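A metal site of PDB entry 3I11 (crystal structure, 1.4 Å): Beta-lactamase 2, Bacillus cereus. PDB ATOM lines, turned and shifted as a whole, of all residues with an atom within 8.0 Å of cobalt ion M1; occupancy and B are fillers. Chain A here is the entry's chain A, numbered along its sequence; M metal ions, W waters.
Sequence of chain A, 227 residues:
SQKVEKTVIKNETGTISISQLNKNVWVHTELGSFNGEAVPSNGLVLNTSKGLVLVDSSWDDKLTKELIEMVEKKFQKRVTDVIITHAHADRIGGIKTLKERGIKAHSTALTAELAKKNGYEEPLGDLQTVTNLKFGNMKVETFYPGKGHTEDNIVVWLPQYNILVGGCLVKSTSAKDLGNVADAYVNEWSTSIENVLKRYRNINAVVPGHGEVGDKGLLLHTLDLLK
NE2 of His 88 sits at hydrogen-bond distance from OD2 of Asp 183, 2.7 Å away.
N of His 149 is in hydrogen-bond range of OD1 of Asn 153, at 2.8 Å.
The guanidinium group (NE) of Arg 91 lies close to the side-chain carboxylate (OD2) of Asp 90 (3.1 Å).
ND1 of His 88 binds cobalt ion M1 (2.0 Å).
Cobalt ion M1 is bound by water W1.
Cobalt ion M1 is bound by NE2 of His 149.
NE2 of His 86 is bound to cobalt ion M1, at 2.1 Å.
Slightly farther from cobalt ion M1 lies water W2 (2.7 Å).
OD1 of Asp 90 touches cobalt ion M1, 3.9 Å away.
Four residues have an atom within 4 Å of cobalt ion M1: His 86, His 88, Asp 90 and His 149.
Along chain A the residues within 4 Å of cobalt ion M1 span positions 86 to 149.
The nearest printed residue that does not touch cobalt ion M1 is Thr 150 (4.2 Å).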
ATOM      1  N   TRP A  59      15.447  25.802  -5.228  1.00  0.00           N
ATOM      2  CA  TRP A  59      15.740  25.180  -3.947  1.00  0.00           C
ATOM      3  C   TRP A  59      15.306  25.946  -2.717  1.00  0.00           C
ATOM      4  O   TRP A  59      15.025  25.354  -1.684  1.00  0.00           O
ATOM      5  CB  TRP A  59      17.298  24.962  -3.786  1.00  0.00           C
ATOM      6  CG  TRP A  59      17.890  24.012  -4.818  1.00  0.00           C
ATOM      7  CD1 TRP A  59      18.421  24.304  -6.040  1.00  0.00           C
ATOM      8  CD2 TRP A  59      18.015  22.576  -4.663  1.00  0.00           C
ATOM      9  NE1 TRP A  59      18.850  23.142  -6.669  1.00  0.00           N
ATOM     10  CE2 TRP A  59      18.603  22.077  -5.835  1.00  0.00           C
ATOM     11  CE3 TRP A  59      17.657  21.678  -3.640  1.00  0.00           C
ATOM     12  CZ2 TRP A  59      18.875  20.686  -6.017  1.00  0.00           C
ATOM     13  CZ3 TRP A  59      17.908  20.295  -3.832  1.00  0.00           C
ATOM     14  CH2 TRP A  59      18.512  19.828  -5.030  1.00  0.00           C
ATOM     15  N   THR A  85       5.831  20.680  -9.162  1.00  0.00           N
ATOM     16  CA  THR A  85       5.678  19.292  -9.584  1.00  0.00           C
ATOM     17  C   THR A  85       5.730  18.227  -8.489  1.00  0.00           C
ATOM     18  O   THR A  85       5.295  17.109  -8.726  1.00  0.00           O
ATOM     19  CB  THR A  85       6.579  18.931 -10.768  1.00  0.00           C
ATOM     20  OG1 THR A  85       7.945  19.018 -10.364  1.00  0.00           O
ATOM     21  CG2 THR A  85       6.305  19.830 -12.041  1.00  0.00           C
ATOM     22  N   HIS A  86       6.265  18.558  -7.323  1.00  0.00           N
ATOM     23  CA  HIS A  86       6.066  17.818  -6.093  1.00  0.00           C
ATOM     24  C   HIS A  86       6.556  18.636  -4.903  1.00  0.00           C
ATOM     25  O   HIS A  86       7.012  19.744  -5.091  1.00  0.00           O
ATOM     26  CB  HIS A  86       6.670  16.423  -6.113  1.00  0.00           C
ATOM     27  CG  HIS A  86       8.170  16.348  -6.066  1.00  0.00           C
ATOM     28  ND1 HIS A  86       8.920  16.478  -7.229  1.00  0.00           N
ATOM     29  CD2 HIS A  86       9.061  16.032  -5.094  1.00  0.00           C
ATOM     30  CE1 HIS A  86      10.193  16.294  -6.952  1.00  0.00           C
ATOM     31  NE2 HIS A  86      10.319  16.044  -5.662  1.00  0.00           N
ATOM     32  N   ALA A  87       6.259  18.139  -3.691  1.00  0.00           N
ATOM     33  CA  ALA A  87       6.406  18.899  -2.448  1.00  0.00           C
ATOM     34  C   ALA A  87       7.734  18.911  -1.777  1.00  0.00           C
ATOM     35  O   ALA A  87       7.887  19.509  -0.695  1.00  0.00           O
ATOM     36  CB  ALA A  87       5.317  18.423  -1.446  1.00  0.00           C
ATOM     37  N   HIS A  88       8.748  18.351  -2.382  1.00  0.00           N
ATOM     38  CA  HIS A  88      10.100  18.348  -1.813  1.00  0.00           C
ATOM     39  C   HIS A  88      10.698  19.737  -1.872  1.00  0.00           C
ATOM     40  O   HIS A  88      10.417  20.534  -2.735  1.00  0.00           O
ATOM     41  CB  HIS A  88      11.028  17.413  -2.569  1.00  0.00           C
ATOM     42  CG  HIS A  88      10.980  16.000  -2.098  1.00  0.00           C
ATOM     43  ND1 HIS A  88      11.511  14.950  -2.846  1.00  0.00           N
ATOM     44  CD2 HIS A  88      10.491  15.430  -0.970  1.00  0.00           C
ATOM     45  CE1 HIS A  88      11.368  13.833  -2.179  1.00  0.00           C
ATOM     46  NE2 HIS A  88      10.734  14.085  -1.055  1.00  0.00           N
ATOM     47  N   ALA A  89      11.611  19.977  -0.912  1.00  0.00           N
ATOM     48  CA  ALA A  89      12.321  21.281  -0.859  1.00  0.00           C
ATOM     49  C   ALA A  89      12.843  21.817  -2.201  1.00  0.00           C
ATOM     50  O   ALA A  89      12.707  23.011  -2.445  1.00  0.00           O
ATOM     51  CB  ALA A  89      13.490  21.209   0.126  1.00  0.00           C
ATOM     52  N   ASP A  90      13.477  21.006  -3.074  1.00  0.00           N
ATOM     53  CA  ASP A  90      13.998  21.504  -4.403  1.00  0.00           C
ATOM     54  C   ASP A  90      12.976  22.076  -5.328  1.00  0.00           C
ATOM     55  O   ASP A  90      13.319  22.793  -6.236  1.00  0.00           O
ATOM     56  CB  ASP A  90      14.869  20.504  -5.232  1.00  0.00           C
ATOM     57  CG  ASP A  90      14.150  19.236  -5.641  1.00  0.00           C
ATOM     58  OD1 ASP A  90      13.512  18.673  -4.732  1.00  0.00           O
ATOM     59  OD2 ASP A  90      14.334  18.732  -6.796  1.00  0.00           O
ATOM     60  N   ARG A  91      11.705  21.711  -5.110  1.00  0.00           N
ATOM     61  CA  ARG A  91      10.570  22.136  -5.956  1.00  0.00           C
ATOM     62  C   ARG A  91       9.749  23.217  -5.255  1.00  0.00           C
ATOM     63  O   ARG A  91       9.326  24.145  -5.916  1.00  0.00           O
ATOM     64  CB  ARG A  91       9.658  20.932  -6.302  1.00  0.00           C
ATOM     65  CG  ARG A  91      10.420  19.818  -7.018  1.00  0.00           C
ATOM     66  CD  ARG A  91      11.422  20.507  -8.058  1.00  0.00           C
ATOM     67  NE  ARG A  91      12.173  19.595  -8.865  1.00  0.00           N
ATOM     68  CZ  ARG A  91      12.854  19.942  -9.965  1.00  0.00           C
ATOM     69  NH1 ARG A  91      12.973  21.211 -10.353  1.00  0.00           N
ATOM     70  NH2 ARG A  91      13.539  19.043 -10.623  1.00  0.00           N
ATOM     71  N   HIS A 149       8.955   8.770  -7.737  1.00  0.00           N
ATOM     72  CA  HIS A 149       9.996   9.440  -6.954  1.00  0.00           C
ATOM     73  C   HIS A 149       9.420   9.935  -5.609  1.00  0.00           C
ATOM     74  O   HIS A 149      10.021   9.800  -4.556  1.00  0.00           O
ATOM     75  CB  HIS A 149      10.528  10.631  -7.780  1.00  0.00           C
ATOM     76  CG  HIS A 149      11.292  11.597  -6.948  1.00  0.00           C
ATOM     77  ND1 HIS A 149      12.567  11.336  -6.465  1.00  0.00           N
ATOM     78  CD2 HIS A 149      10.939  12.800  -6.464  1.00  0.00           C
ATOM     79  CE1 HIS A 149      12.941  12.326  -5.687  1.00  0.00           C
ATOM     80  NE2 HIS A 149      11.987  13.260  -5.707  1.00  0.00           N
ATOM     81  N   THR A 150       8.167  10.426  -5.670  1.00  0.00           N
ATOM     82  CA  THR A 150       7.372  10.691  -4.505  1.00  0.00           C
ATOM     83  C   THR A 150       5.916  10.245  -4.795  1.00  0.00           C
ATOM     84  O   THR A 150       5.563   9.868  -5.911  1.00  0.00           O
ATOM     85  CB  THR A 150       7.367  12.177  -4.160  1.00  0.00           C
ATOM     86  OG1 THR A 150       6.802  12.895  -5.265  1.00  0.00           O
ATOM     87  CG2 THR A 150       8.732  12.675  -3.732  1.00  0.00           C
ATOM     88  N   ASP A 152       3.355  12.132  -4.880  1.00  0.00           N
ATOM     89  CA  ASP A 152       2.613  13.243  -5.489  1.00  0.00           C
ATOM     90  C   ASP A 152       3.123  13.702  -6.842  1.00  0.00           C
ATOM     91  O   ASP A 152       2.492  14.561  -7.460  1.00  0.00           O
ATOM     92  CB  ASP A 152       2.509  14.438  -4.560  1.00  0.00           C
ATOM     93  CG  ASP A 152       3.858  15.039  -4.174  1.00  0.00           C
ATOM     94  OD1 ASP A 152       4.846  14.290  -3.920  1.00  0.00           O
ATOM     95  OD2 ASP A 152       3.933  16.279  -4.131  1.00  0.00           O
ATOM     96  N   ASN A 153       4.279  13.177  -7.295  1.00  0.00           N
ATOM     97  CA  ASN A 153       4.934  13.717  -8.481  1.00  0.00           C
ATOM     98  C   ASN A 153       4.035  13.804  -9.688  1.00  0.00           C
ATOM     99  O   ASN A 153       3.274  12.872 -10.053  1.00  0.00           O
ATOM    100  CB  ASN A 153       6.228  12.967  -8.827  1.00  0.00           C
ATOM    101  CG  ASN A 153       6.149  11.444  -8.863  1.00  0.00           C
ATOM    102  OD1 ASN A 153       7.186  10.806  -8.620  1.00  0.00           O
ATOM    103  ND2 ASN A 153       5.016  10.857  -9.176  1.00  0.00           N
ATOM    104  N   GLY A 167      10.361  16.022 -14.405  1.00  0.00           N
ATOM    105  CA  GLY A 167      10.696  16.204 -12.996  1.00  0.00           C
ATOM    106  C   GLY A 167      11.462  15.040 -12.416  1.00  0.00           C
ATOM    107  O   GLY A 167      12.112  14.289 -13.138  1.00  0.00           O
ATOM    108  N   CYS A 168      11.446  14.886 -11.083  1.00  0.00           N
ATOM    109  CA  CYS A 168      12.262  13.837 -10.529  1.00  0.00           C
ATOM    110  C   CYS A 168      11.722  12.419 -10.763  1.00  0.00           C
ATOM    111  O   CYS A 168      12.434  11.454 -10.502  1.00  0.00           O
ATOM    112  CB  CYS A 168      12.596  14.092  -9.063  1.00  0.00           C
ATOM    113  SG  CYS A 168      13.535  15.661  -8.852  1.00  0.00           S
ATOM    114  N   LEU A 169      10.491  12.295 -11.311  1.00  0.00           N
ATOM    115  CA  LEU A 169      10.051  11.024 -11.809  1.00  0.00           C
ATOM    116  C   LEU A 169      10.984  10.423 -12.883  1.00  0.00           C
ATOM    117  O   LEU A 169      11.032   9.196 -13.087  1.00  0.00           O
ATOM    118  CB  LEU A 169       8.646  11.184 -12.392  1.00  0.00           C
ATOM    119  CG  LEU A 169       7.919   9.919 -12.795  1.00  0.00           C
ATOM    120  CD1 LEU A 169       7.419   9.117 -11.572  1.00  0.00           C
ATOM    121  CD2 LEU A 169       6.735  10.291 -13.740  1.00  0.00           C
ATOM    122  N   ASN A 180      17.486   9.766  -4.082  1.00  0.00           N
ATOM    123  CA  ASN A 180      16.774   9.727  -2.802  1.00  0.00           C
ATOM    124  C   ASN A 180      15.473   8.962  -2.917  1.00  0.00           C
ATOM    125  O   ASN A 180      14.523   9.492  -3.525  1.00  0.00           O
ATOM    126  CB  ASN A 180      16.471  11.156  -2.331  1.00  0.00           C
ATOM    127  CG  ASN A 180      15.581  11.213  -1.074  1.00  0.00           C
ATOM    128  OD1 ASN A 180      15.547  10.274  -0.242  1.00  0.00           O
ATOM    129  ND2 ASN A 180      14.812  12.309  -0.965  1.00  0.00           N
ATOM    130  N   ASP A 183      11.274   8.799   0.133  1.00  0.00           N
ATOM    131  CA  ASP A 183       9.892   9.129  -0.076  1.00  0.00           C
ATOM    132  C   ASP A 183       9.319   8.489  -1.344  1.00  0.00           C
ATOM    133  O   ASP A 183       8.200   8.832  -1.782  1.00  0.00           O
ATOM    134  CB  ASP A 183       9.748  10.651  -0.140  1.00  0.00           C
ATOM    135  CG  ASP A 183      10.061  11.310   1.174  1.00  0.00           C
ATOM    136  OD1 ASP A 183       9.777  10.748   2.265  1.00  0.00           O
ATOM    137  OD2 ASP A 183      10.605  12.421   1.101  1.00  0.00           O
ATOM    138  N   HIS A 210      16.726  16.545 -12.916  1.00  0.00           N
ATOM    139  CA  HIS A 210      18.137  16.918 -12.784  1.00  0.00           C
ATOM    140  C   HIS A 210      18.876  16.376 -14.024  1.00  0.00           C
ATOM    141  O   HIS A 210      18.604  15.268 -14.483  1.00  0.00           O
ATOM    142  CB  HIS A 210      18.701  16.320 -11.481  1.00  0.00           C
ATOM    143  CG  HIS A 210      17.890  16.621 -10.244  1.00  0.00           C
ATOM    144  ND1 HIS A 210      18.102  17.735  -9.440  1.00  0.00           N
ATOM    145  CD2 HIS A 210      16.859  15.947  -9.657  1.00  0.00           C
ATOM    146  CE1 HIS A 210      17.263  17.727  -8.425  1.00  0.00           C
ATOM    147  NE2 HIS A 210      16.474  16.662  -8.534  1.00  0.00           N
HETATM  148 CO    CO M   1      12.001  15.087  -4.798  1.00  0.00          CO
HETATM  149 CO    CO M   2      14.416  16.263  -7.400  1.00  0.00          CO
HETATM  150  O   HOH W   1      13.612  16.231  -5.286  1.00  0.00           O
HETATM  151  O   HOH W   2      14.304  14.231  -3.578  1.00  0.00           O
